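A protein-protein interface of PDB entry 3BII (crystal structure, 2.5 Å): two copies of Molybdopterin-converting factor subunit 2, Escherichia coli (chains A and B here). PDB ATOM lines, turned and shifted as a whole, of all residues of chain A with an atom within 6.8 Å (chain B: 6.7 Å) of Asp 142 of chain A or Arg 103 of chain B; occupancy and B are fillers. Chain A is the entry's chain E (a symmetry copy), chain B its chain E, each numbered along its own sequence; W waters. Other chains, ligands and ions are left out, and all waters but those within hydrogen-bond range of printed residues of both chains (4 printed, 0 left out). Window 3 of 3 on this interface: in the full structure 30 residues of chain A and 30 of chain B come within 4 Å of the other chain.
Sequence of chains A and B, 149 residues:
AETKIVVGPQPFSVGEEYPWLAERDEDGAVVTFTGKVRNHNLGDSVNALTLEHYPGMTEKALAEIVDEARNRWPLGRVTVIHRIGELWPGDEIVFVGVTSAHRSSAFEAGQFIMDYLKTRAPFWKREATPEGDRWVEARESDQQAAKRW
No position is printed for both chains.
CB of Ala 29 of chain B touches CE1 of Phe 33 of chain A, at 3.8 Å.
Phe 33 of chain A touches Val 30 of chain B (CA to O, 3.3 Å).
Phe 33 of chain A touches Val 31 of chain B.
CE1 of Phe 33 of chain A touches CB of Arg 103 of chain B, at 3.3 Å.
Phe 33 of chain A touches Phe 107 of chain B (CB to CZ, 3.7 Å).
NH2 of Arg 38 of chain A touches CA of His 102 of chain B (3.8 Å).
Phe 107 of chain B touches Gln 111 of chain A (CG to CG, 3.4 Å).
Met 114 of chain A touches Arg 103 of chain B.
NH1 of Arg 103 of chain B touches CD of Lys 118 of chain A, 3.2 Å away.
The backbone carbonyl oxygen (O) of His 102 of chain B lies within hydrogen-bond range of the side-chain hydroxyl (OG) of Ser 105 of chain B, at 3.4 Å.
The backbone NH of Gly 28 of chain B sits at hydrogen-bond distance from the backbone carbonyl oxygen of Ser 100 of chain B, at 3.3 Å.
The backbone carbonyl oxygen (O) of Ser 100 of chain B is in hydrogen-bond range of the backbone NH (N) of Ala 29 of chain B.
A ring nitrogen (ND1) of His 102 of chain B sits at hydrogen-bond distance from the side-chain hydroxyl of Ser 104 of chain B, 2.9 Å away.
O of Asp 115 of chain A sits at hydrogen-bond distance from OG1 of Thr 119 of chain A.
NH2 of Arg 148 of chain A lies within salt-bridge range of OD2 of Asp 115 of chain A, at 3.0 Å.
The guanidinium group (NH2) of Arg 103 of chain B lies within salt-bridge range of the side-chain carboxylate (OD1) of Asp 115 of chain A (2.8 Å).
O of Ala 101 of chain B lies within hydrogen-bond range of NH2 of Arg 38 of chain A, 2.6 Å away.
O of Gly 28 of chain B lies within hydrogen-bond range of NH1 of Arg 38 of chain A, 3.2 Å away.
The guanidinium group of Arg 103 of chain B lies within salt-bridge range of the side-chain carboxylate of Asp 142 of chain A, 3.0 Å away.
Hydrophobic or aromatic side chains of chain B within 4 Å of the printed part of chain A: Ala 29, Val 31 and Phe 107.
Printed residues of chain A that touch a printed residue of chain B: Phe 33, Arg 38, Gln 111, Met 114, Asp 115, Lys 118 and Asp 142.
Hydrophobic or aromatic side chains of chain A that line the printed part of chain B: Phe 33 and Met 114.
Among the printed residues, 13 pairs touch across the chains.
Among the printed residues, Asp or Glu carboxylates within 4 Å of a Lys or Arg side-chain nitrogen of the other chain: Asp 115 of chain A with Arg 103 of chain B and Asp 142 of chain A with Arg 103 of chain B.
Water W4 lies within hydrogen-bond range of the side-chain carboxylate of Asp 115 of chain A and the guanidinium group of Arg 103 of chain B.
Water W2 lies within hydrogen-bond range of the side-chain carboxylate (OD1) of Asp 142 of chain A (2.5 Å), the side-chain hydroxyl (OG) of Ser 141 of chain A (2.8 Å) and a ring nitrogen (NE2) of His 102 of chain B (3.1 Å).
Water W1 lies within hydrogen-bond range of O of Asp 115 of chain A, O of Asp 142 of chain A and NH2 of Arg 103 of chain B.
Water W3 lies within hydrogen-bond range of OD1 of Asp 115 of chain A (2.7 Å), O of Gln 111 of chain A (2.9 Å) and NE of Arg 103 of chain B (2.9 Å).
Of the printed residues of chain B, Gln 111 of chain A touches Phe 107.
Of the printed residues of chain B, Asp 142 of chain A touches Arg 103 (3.0 Å).
Printed residues of chain A within 4 Å of Ala 29 of chain B: Phe 33.
Of the printed residues of chain A, Val 30 of chain B touches Phe 33.
Of the printed residues of chain A, Val 31 of chain B touches Phe 33.
Of the printed residues of chain A, Phe 107 of chain B touches Phe 33 (3.7 Å) and Gln 111 (3.4 Å).
The nearest residue of chain B that does not touch Asp 142 of chain A is His 102 of chain B (4.6 Å).
The nearest printed residue of chain B that does not touch Arg 38 of chain A is Ala 29 of chain B (4.05 Å).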
ATOM      1  N   PHE A  33       0.943  14.627  33.330  1.00  0.00           N
ATOM      2  CA  PHE A  33       0.107  15.745  32.925  1.00  0.00           C
ATOM      3  C   PHE A  33      -0.956  15.267  31.929  1.00  0.00           C
ATOM      4  O   PHE A  33      -0.666  14.489  31.034  1.00  0.00           O
ATOM      5  CB  PHE A  33       0.923  16.903  32.318  1.00  0.00           C
ATOM      6  CG  PHE A  33       0.060  18.022  31.741  1.00  0.00           C
ATOM      7  CD1 PHE A  33      -0.332  19.098  32.545  1.00  0.00           C
ATOM      8  CD2 PHE A  33      -0.386  17.972  30.407  1.00  0.00           C
ATOM      9  CE1 PHE A  33      -1.143  20.126  32.045  1.00  0.00           C
ATOM     10  CE2 PHE A  33      -1.206  19.016  29.883  1.00  0.00           C
ATOM     11  CZ  PHE A  33      -1.583  20.102  30.717  1.00  0.00           C
ATOM     12  N   ARG A  38     -10.689  22.590  25.799  1.00  0.00           N
ATOM     13  CA  ARG A  38     -11.309  23.712  26.538  1.00  0.00           C
ATOM     14  C   ARG A  38     -12.602  24.181  25.841  1.00  0.00           C
ATOM     15  O   ARG A  38     -12.691  24.152  24.603  1.00  0.00           O
ATOM     16  CB  ARG A  38     -10.324  24.890  26.653  1.00  0.00           C
ATOM     17  CG  ARG A  38      -8.838  24.499  26.862  1.00  0.00           C
ATOM     18  CD  ARG A  38      -8.608  23.595  28.120  1.00  0.00           C
ATOM     19  NE  ARG A  38      -7.460  24.051  28.927  1.00  0.00           N
ATOM     20  CZ  ARG A  38      -6.262  23.449  29.011  1.00  0.00           C
ATOM     21  NH1 ARG A  38      -5.981  22.297  28.363  1.00  0.00           N
ATOM     22  NH2 ARG A  38      -5.333  23.999  29.773  1.00  0.00           N
ATOM     23  N   GLN A 111       7.002  19.705  32.456  1.00  0.00           N
ATOM     24  CA  GLN A 111       6.743  21.080  32.007  1.00  0.00           C
ATOM     25  C   GLN A 111       7.408  21.372  30.680  1.00  0.00           C
ATOM     26  O   GLN A 111       6.774  21.921  29.778  1.00  0.00           O
ATOM     27  CB  GLN A 111       7.289  22.080  33.023  1.00  0.00           C
ATOM     28  CG  GLN A 111       6.587  22.028  34.364  1.00  0.00           C
ATOM     29  CD  GLN A 111       7.182  22.991  35.374  1.00  0.00           C
ATOM     30  OE1 GLN A 111       6.674  24.108  35.547  1.00  0.00           O
ATOM     31  NE2 GLN A 111       8.267  22.575  36.038  1.00  0.00           N
ATOM     32  N   MET A 114       5.712  19.587  27.738  1.00  0.00           N
ATOM     33  CA  MET A 114       4.479  20.247  27.291  1.00  0.00           C
ATOM     34  C   MET A 114       4.770  21.553  26.551  1.00  0.00           C
ATOM     35  O   MET A 114       4.200  21.786  25.485  1.00  0.00           O
ATOM     36  CB  MET A 114       3.495  20.431  28.430  1.00  0.00           C
ATOM     37  CG  MET A 114       2.799  19.126  28.791  1.00  0.00           C
ATOM     38  SD  MET A 114       1.698  18.534  27.464  1.00  0.00           S
ATOM     39  CE  MET A 114       0.914  20.081  26.982  1.00  0.00           C
ATOM     40  N   ASP A 115       5.670  22.391  27.076  1.00  0.00           N
ATOM     41  CA  ASP A 115       5.967  23.664  26.406  1.00  0.00           C
ATOM     42  C   ASP A 115       6.556  23.480  25.004  1.00  0.00           C
ATOM     43  O   ASP A 115       6.303  24.296  24.102  1.00  0.00           O
ATOM     44  CB  ASP A 115       6.992  24.481  27.199  1.00  0.00           C
ATOM     45  CG  ASP A 115       6.441  25.078  28.480  1.00  0.00           C
ATOM     46  OD1 ASP A 115       5.191  25.175  28.669  1.00  0.00           O
ATOM     47  OD2 ASP A 115       7.310  25.471  29.280  1.00  0.00           O
ATOM     48  N   TYR A 116       7.372  22.445  24.825  1.00  0.00           N
ATOM     49  CA  TYR A 116       7.907  22.155  23.498  1.00  0.00           C
ATOM     50  C   TYR A 116       6.871  21.478  22.582  1.00  0.00           C
ATOM     51  O   TYR A 116       6.791  21.769  21.388  1.00  0.00           O
ATOM     52  CB  TYR A 116       9.191  21.326  23.590  1.00  0.00           C
ATOM     53  CG  TYR A 116      10.485  22.135  23.663  1.00  0.00           C
ATOM     54  CD1 TYR A 116      11.667  21.657  23.060  1.00  0.00           C
ATOM     55  CD2 TYR A 116      10.534  23.372  24.322  1.00  0.00           C
ATOM     56  CE1 TYR A 116      12.833  22.371  23.126  1.00  0.00           C
ATOM     57  CE2 TYR A 116      11.701  24.104  24.385  1.00  0.00           C
ATOM     58  CZ  TYR A 116      12.854  23.598  23.788  1.00  0.00           C
ATOM     59  OH  TYR A 116      14.026  24.335  23.843  1.00  0.00           O
ATOM     60  N   LYS A 118       3.679  22.056  22.595  1.00  0.00           N
ATOM     61  CA  LYS A 118       2.751  23.124  22.214  1.00  0.00           C
ATOM     62  C   LYS A 118       3.317  24.155  21.241  1.00  0.00           C
ATOM     63  O   LYS A 118       2.575  24.994  20.746  1.00  0.00           O
ATOM     64  CB  LYS A 118       2.259  23.861  23.462  1.00  0.00           C
ATOM     65  CG  LYS A 118       1.103  23.165  24.176  1.00  0.00           C
ATOM     66  CD  LYS A 118       0.289  24.168  24.981  1.00  0.00           C
ATOM     67  CE  LYS A 118      -0.988  23.535  25.488  1.00  0.00           C
ATOM     68  NZ  LYS A 118      -2.065  23.587  24.469  1.00  0.00           N
ATOM     69  N   THR A 119       4.622  24.151  21.007  1.00  0.00           N
ATOM     70  CA  THR A 119       5.182  25.069  20.006  1.00  0.00           C
ATOM     71  C   THR A 119       5.943  24.350  18.877  1.00  0.00           C
ATOM     72  O   THR A 119       6.337  24.996  17.913  1.00  0.00           O
ATOM     73  CB  THR A 119       6.093  26.117  20.628  1.00  0.00           C
ATOM     74  OG1 THR A 119       7.158  25.468  21.335  1.00  0.00           O
ATOM     75  CG2 THR A 119       5.304  27.013  21.567  1.00  0.00           C
ATOM     76  N   GLU A 137      -6.276  30.056  17.754  1.00  0.00           N
ATOM     77  CA  GLU A 137      -5.158  30.953  17.690  1.00  0.00           C
ATOM     78  C   GLU A 137      -4.008  30.422  18.547  1.00  0.00           C
ATOM     79  O   GLU A 137      -4.228  29.860  19.609  1.00  0.00           O
ATOM     80  CB  GLU A 137      -5.598  32.341  18.159  1.00  0.00           C
ATOM     81  CG  GLU A 137      -4.721  33.526  17.672  1.00  0.00           C
ATOM     82  CD  GLU A 137      -4.890  33.835  16.181  1.00  0.00           C
ATOM     83  OE1 GLU A 137      -6.005  33.627  15.652  1.00  0.00           O
ATOM     84  OE2 GLU A 137      -3.905  34.290  15.549  1.00  0.00           O
ATOM     85  N   ALA A 138      -2.786  30.565  18.043  1.00  0.00           N
ATOM     86  CA  ALA A 138      -1.559  30.220  18.789  1.00  0.00           C
ATOM     87  C   ALA A 138      -1.188  31.346  19.758  1.00  0.00           C
ATOM     88  O   ALA A 138      -1.173  32.502  19.354  1.00  0.00           O
ATOM     89  CB  ALA A 138      -0.404  29.946  17.831  1.00  0.00           C
ATOM     90  N   ARG A 139      -0.885  30.998  21.013  1.00  0.00           N
ATOM     91  CA  ARG A 139      -0.586  31.957  22.085  1.00  0.00           C
ATOM     92  C   ARG A 139       0.862  32.401  22.238  1.00  0.00           C
ATOM     93  O   ARG A 139       1.803  31.595  22.295  1.00  0.00           O
ATOM     94  CB  ARG A 139      -1.058  31.420  23.430  1.00  0.00           C
ATOM     95  CG  ARG A 139      -2.530  31.216  23.464  1.00  0.00           C
ATOM     96  CD  ARG A 139      -2.956  30.496  24.717  1.00  0.00           C
ATOM     97  NE  ARG A 139      -4.401  30.272  24.693  1.00  0.00           N
ATOM     98  CZ  ARG A 139      -5.095  29.640  25.641  1.00  0.00           C
ATOM     99  NH1 ARG A 139      -4.493  29.132  26.719  1.00  0.00           N
ATOM    100  NH2 ARG A 139      -6.411  29.506  25.498  1.00  0.00           N
ATOM    101  N   GLU A 140       1.019  33.708  22.368  1.00  0.00           N
ATOM    102  CA  GLU A 140       2.297  34.317  22.698  1.00  0.00           C
ATOM    103  C   GLU A 140       2.874  33.772  24.008  1.00  0.00           C
ATOM    104  O   GLU A 140       4.094  33.698  24.161  1.00  0.00           O
ATOM    105  CB  GLU A 140       2.131  35.849  22.737  1.00  0.00           C
ATOM    106  CG  GLU A 140       3.355  36.695  23.116  1.00  0.00           C
ATOM    107  CD  GLU A 140       4.615  36.405  22.297  1.00  0.00           C
ATOM    108  OE1 GLU A 140       4.513  36.037  21.101  1.00  0.00           O
ATOM    109  OE2 GLU A 140       5.725  36.548  22.870  1.00  0.00           O
ATOM    110  N   SER A 141       2.012  33.398  24.949  1.00  0.00           N
ATOM    111  CA  SER A 141       2.498  32.863  26.236  1.00  0.00           C
ATOM    112  C   SER A 141       3.141  31.460  26.120  1.00  0.00           C
ATOM    113  O   SER A 141       4.003  31.116  26.936  1.00  0.00           O
ATOM    114  CB  SER A 141       1.433  32.908  27.346  1.00  0.00           C
ATOM    115  OG  SER A 141       0.316  32.072  27.058  1.00  0.00           O
ATOM    116  N   ASP A 142       2.750  30.683  25.104  1.00  0.00           N
ATOM    117  CA  ASP A 142       3.393  29.397  24.834  1.00  0.00           C
ATOM    118  C   ASP A 142       4.779  29.573  24.239  1.00  0.00           C
ATOM    119  O   ASP A 142       5.693  28.806  24.540  1.00  0.00           O
ATOM    120  CB  ASP A 142       2.523  28.520  23.931  1.00  0.00           C
ATOM    121  CG  ASP A 142       1.255  28.035  24.626  1.00  0.00           C
ATOM    122  OD1 ASP A 142       1.201  28.002  25.874  1.00  0.00           O
ATOM    123  OD2 ASP A 142       0.301  27.682  23.907  1.00  0.00           O
ATOM    124  N   GLN A 143       4.931  30.608  23.420  1.00  0.00           N
ATOM    125  CA  GLN A 143       6.243  31.002  22.883  1.00  0.00           C
ATOM    126  C   GLN A 143       7.187  31.495  23.969  1.00  0.00           C
ATOM    127  O   GLN A 143       8.390  31.208  23.928  1.00  0.00           O
ATOM    128  CB  GLN A 143       6.113  32.086  21.816  1.00  0.00           C
ATOM    129  CG  GLN A 143       5.268  31.712  20.608  1.00  0.00           C
ATOM    130  CD  GLN A 143       5.988  30.800  19.672  1.00  0.00           C
ATOM    131  OE1 GLN A 143       5.406  29.845  19.159  1.00  0.00           O
ATOM    132  NE2 GLN A 143       7.276  31.062  19.457  1.00  0.00           N
ATOM    133  N   GLN A 144       6.658  32.238  24.936  1.00  0.00           N
ATOM    134  CA  GLN A 144       7.503  32.675  26.039  1.00  0.00           C
ATOM    135  C   GLN A 144       7.860  31.514  27.000  1.00  0.00           C
ATOM    136  O   GLN A 144       9.000  31.399  27.462  1.00  0.00           O
ATOM    137  CB  GLN A 144       6.957  33.947  26.723  1.00  0.00           C
ATOM    138  CG  GLN A 144       7.100  35.246  25.833  1.00  0.00           C
ATOM    139  CD  GLN A 144       8.504  35.400  25.116  1.00  0.00           C
ATOM    140  OE1 GLN A 144       8.652  35.052  23.920  1.00  0.00           O
ATOM    141  NE2 GLN A 144       9.527  35.911  25.857  1.00  0.00           N
ATOM    142  N   ALA A 145       6.905  30.622  27.230  1.00  0.00           N
ATOM    143  CA  ALA A 145       7.164  29.380  27.945  1.00  0.00           C
ATOM    144  C   ALA A 145       8.271  28.532  27.284  1.00  0.00           C
ATOM    145  O   ALA A 145       9.152  28.025  27.986  1.00  0.00           O
ATOM    146  CB  ALA A 145       5.876  28.569  28.073  1.00  0.00           C
ATOM    147  N   ALA A 146       8.225  28.372  25.950  1.00  0.00           N
ATOM    148  CA  ALA A 146       9.212  27.520  25.241  1.00  0.00           C
ATOM    149  C   ALA A 146      10.607  28.118  25.280  1.00  0.00           C
ATOM    150  O   ALA A 146      11.574  27.418  25.557  1.00  0.00           O
ATOM    151  CB  ALA A 146       8.785  27.224  23.802  1.00  0.00           C
ATOM    152  N   LYS A 147      10.704  29.413  25.013  1.00  0.00           N
ATOM    153  CA  LYS A 147      11.982  30.118  25.029  1.00  0.00           C
ATOM    154  C   LYS A 147      12.684  30.228  26.400  1.00  0.00           C
ATOM    155  O   LYS A 147      13.851  30.571  26.458  1.00  0.00           O
ATOM    156  CB  LYS A 147      11.813  31.510  24.407  1.00  0.00           C
ATOM    157  CG  LYS A 147      11.653  31.465  22.904  1.00  0.00           C
ATOM    158  CD  LYS A 147      10.904  32.674  22.385  1.00  0.00           C
ATOM    159  CE  LYS A 147      10.622  32.531  20.892  1.00  0.00           C
ATOM    160  NZ  LYS A 147      10.316  33.865  20.301  1.00  0.00           N
ATOM    161  N   ARG A 148      11.996  29.951  27.502  1.00  0.00           N
ATOM    162  CA  ARG A 148      12.654  30.072  28.798  1.00  0.00           C
ATOM    163  C   ARG A 148      13.536  28.828  29.028  1.00  0.00           C
ATOM    164  O   ARG A 148      14.484  28.862  29.820  1.00  0.00           O
ATOM    165  CB  ARG A 148      11.643  30.354  29.934  1.00  0.00           C
ATOM    166  CG  ARG A 148      10.901  29.102  30.447  1.00  0.00           C
ATOM    167  CD  ARG A 148       9.532  29.322  31.123  1.00  0.00           C
ATOM    168  NE  ARG A 148       8.959  27.991  31.398  1.00  0.00           N
ATOM    169  CZ  ARG A 148       7.749  27.724  31.913  1.00  0.00           C
ATOM    170  NH1 ARG A 148       6.909  28.707  32.229  1.00  0.00           N
ATOM    171  NH2 ARG A 148       7.368  26.444  32.092  1.00  0.00           N
ATOM    172  N   GLY B  28      -9.262  21.848  32.867  1.00  0.00           N
ATOM    173  CA  GLY B  28      -8.718  21.285  31.647  1.00  0.00           C
ATOM    174  C   GLY B  28      -7.269  20.860  31.724  1.00  0.00           C
ATOM    175  O   GLY B  28      -6.759  20.289  30.757  1.00  0.00           O
ATOM    176  N   ALA B  29      -6.596  21.149  32.842  1.00  0.00           N
ATOM    177  CA  ALA B  29      -5.207  20.736  33.035  1.00  0.00           C
ATOM    178  C   ALA B  29      -5.093  19.902  34.312  1.00  0.00           C
ATOM    179  O   ALA B  29      -5.370  20.392  35.392  1.00  0.00           O
ATOM    180  CB  ALA B  29      -4.284  21.941  33.097  1.00  0.00           C
ATOM    181  N   VAL B  30      -4.692  18.635  34.182  1.00  0.00           N
ATOM    182  CA  VAL B  30      -4.520  17.758  35.344  1.00  0.00           C
ATOM    183  C   VAL B  30      -3.069  17.294  35.531  1.00  0.00           C
ATOM    184  O   VAL B  30      -2.559  16.540  34.718  1.00  0.00           O
ATOM    185  CB  VAL B  30      -5.445  16.504  35.238  1.00  0.00           C
ATOM    186  CG1 VAL B  30      -5.186  15.550  36.385  1.00  0.00           C
ATOM    187  CG2 VAL B  30      -6.919  16.902  35.203  1.00  0.00           C
ATOM    188  N   VAL B  31      -2.423  17.746  36.604  1.00  0.00           N
ATOM    189  CA  VAL B  31      -1.082  17.280  37.004  1.00  0.00           C
ATOM    190  C   VAL B  31      -1.170  16.296  38.165  1.00  0.00           C
ATOM    191  O   VAL B  31      -1.801  16.633  39.147  1.00  0.00           O
ATOM    192  CB  VAL B  31      -0.224  18.484  37.434  1.00  0.00           C
ATOM    193  CG1 VAL B  31       1.081  18.065  38.080  1.00  0.00           C
ATOM    194  CG2 VAL B  31       0.064  19.352  36.211  1.00  0.00           C
ATOM    195  N   SER B 100      -6.529  22.603  37.191  1.00  0.00           N
ATOM    196  CA  SER B 100      -6.638  24.024  36.964  1.00  0.00           C
ATOM    197  C   SER B 100      -6.964  24.212  35.503  1.00  0.00           C
ATOM    198  O   SER B 100      -6.936  23.265  34.737  1.00  0.00           O
ATOM    199  CB  SER B 100      -5.295  24.674  37.300  1.00  0.00           C
ATOM    200  OG  SER B 100      -5.333  26.082  37.236  1.00  0.00           O
ATOM    201  N   ALA B 101      -7.295  25.438  35.119  1.00  0.00           N
ATOM    202  CA  ALA B 101      -7.623  25.750  33.717  1.00  0.00           C
ATOM    203  C   ALA B 101      -6.384  25.734  32.816  1.00  0.00           C
ATOM    204  O   ALA B 101      -6.483  25.401  31.639  1.00  0.00           O
ATOM    205  CB  ALA B 101      -8.308  27.071  33.622  1.00  0.00           C
ATOM    206  N   HIS B 102      -5.222  26.077  33.379  1.00  0.00           N
ATOM    207  CA  HIS B 102      -3.958  26.148  32.620  1.00  0.00           C
ATOM    208  C   HIS B 102      -2.849  25.250  33.236  1.00  0.00           C
ATOM    209  O   HIS B 102      -2.794  25.068  34.452  1.00  0.00           O
ATOM    210  CB  HIS B 102      -3.493  27.592  32.556  1.00  0.00           C
ATOM    211  CG  HIS B 102      -2.460  27.852  31.503  1.00  0.00           C
ATOM    212  ND1 HIS B 102      -1.111  27.615  31.705  1.00  0.00           N
ATOM    213  CD2 HIS B 102      -2.577  28.338  30.242  1.00  0.00           C
ATOM    214  CE1 HIS B 102      -0.447  27.923  30.605  1.00  0.00           C
ATOM    215  NE2 HIS B 102      -1.312  28.364  29.704  1.00  0.00           N
ATOM    216  N   ARG B 103      -1.975  24.694  32.391  1.00  0.00           N
ATOM    217  CA  ARG B 103      -0.861  23.861  32.860  1.00  0.00           C
ATOM    218  C   ARG B 103       0.117  24.562  33.799  1.00  0.00           C
ATOM    219  O   ARG B 103       0.659  23.939  34.744  1.00  0.00           O
ATOM    220  CB  ARG B 103      -0.107  23.222  31.681  1.00  0.00           C
ATOM    221  CG  ARG B 103       0.844  24.123  30.951  1.00  0.00           C
ATOM    222  CD  ARG B 103       1.251  23.499  29.627  1.00  0.00           C
ATOM    223  NE  ARG B 103       2.212  24.331  28.910  1.00  0.00           N
ATOM    224  CZ  ARG B 103       1.853  25.308  28.092  1.00  0.00           C
ATOM    225  NH1 ARG B 103       0.567  25.549  27.894  1.00  0.00           N
ATOM    226  NH2 ARG B 103       2.769  26.042  27.477  1.00  0.00           N
ATOM    227  N   SER B 104       0.360  25.843  33.562  1.00  0.00           N
ATOM    228  CA  SER B 104       1.280  26.540  34.417  1.00  0.00           C
ATOM    229  C   SER B 104       0.859  26.563  35.871  1.00  0.00           C
ATOM    230  O   SER B 104       1.720  26.416  36.713  1.00  0.00           O
ATOM    231  CB  SER B 104       1.561  27.946  33.931  1.00  0.00           C
ATOM    232  OG  SER B 104       0.362  28.675  33.933  1.00  0.00           O
ATOM    233  N   SER B 105      -0.415  26.726  36.207  1.00  0.00           N
ATOM    234  CA  SER B 105      -0.746  26.769  37.643  1.00  0.00           C
ATOM    235  C   SER B 105      -0.847  25.400  38.282  1.00  0.00           C
ATOM    236  O   SER B 105      -0.611  25.210  39.468  1.00  0.00           O
ATOM    237  CB  SER B 105      -2.001  27.593  37.902  1.00  0.00           C
ATOM    238  OG  SER B 105      -3.127  27.066  37.226  1.00  0.00           O
ATOM    239  N   ALA B 106      -1.184  24.433  37.463  1.00  0.00           N
ATOM    240  CA  ALA B 106      -1.289  23.033  37.911  1.00  0.00           C
ATOM    241  C   ALA B 106       0.075  22.403  38.257  1.00  0.00           C
ATOM    242  O   ALA B 106       0.237  21.847  39.335  1.00  0.00           O
ATOM    243  CB  ALA B 106      -2.033  22.182  36.879  1.00  0.00           C
ATOM    244  N   PHE B 107       1.045  22.498  37.343  1.00  0.00           N
ATOM    245  CA  PHE B 107       2.442  22.140  37.638  1.00  0.00           C
ATOM    246  C   PHE B 107       2.997  22.895  38.836  1.00  0.00           C
ATOM    247  O   PHE B 107       3.599  22.277  39.713  1.00  0.00           O
ATOM    248  CB  PHE B 107       3.351  22.426  36.460  1.00  0.00           C
ATOM    249  CG  PHE B 107       3.394  21.343  35.447  1.00  0.00           C
ATOM    250  CD1 PHE B 107       2.974  21.587  34.140  1.00  0.00           C
ATOM    251  CD2 PHE B 107       3.911  20.071  35.770  1.00  0.00           C
ATOM    252  CE1 PHE B 107       3.055  20.551  33.163  1.00  0.00           C
ATOM    253  CE2 PHE B 107       3.966  19.035  34.816  1.00  0.00           C
ATOM    254  CZ  PHE B 107       3.548  19.273  33.506  1.00  0.00           C
ATOM    255  N   GLU B 108       2.822  24.222  38.873  1.00  0.00           N
ATOM    256  CA  GLU B 108       3.322  25.017  39.997  1.00  0.00           C
ATOM    257  C   GLU B 108       2.693  24.612  41.324  1.00  0.00           C
ATOM    258  O   GLU B 108       3.423  24.325  42.258  1.00  0.00           O
ATOM    259  CB  GLU B 108       3.126  26.498  39.770  1.00  0.00           C
ATOM    260  CG  GLU B 108       4.164  27.146  38.854  1.00  0.00           C
ATOM    261  CD  GLU B 108       3.684  28.509  38.297  1.00  0.00           C
ATOM    262  OE1 GLU B 108       2.819  29.181  38.913  1.00  0.00           O
ATOM    263  OE2 GLU B 108       4.166  28.913  37.223  1.00  0.00           O
HETATM  264  O   HOH W   1       4.856  26.308  25.074  1.00  0.00           O
HETATM  265  O   HOH W   2       0.983  29.488  27.882  1.00  0.00           O
HETATM  266  O   HOH W   3       4.412  23.355  30.531  1.00  0.00           O
HETATM  267  O   HOH W   4       4.209  26.460  30.516  1.00  0.00           O
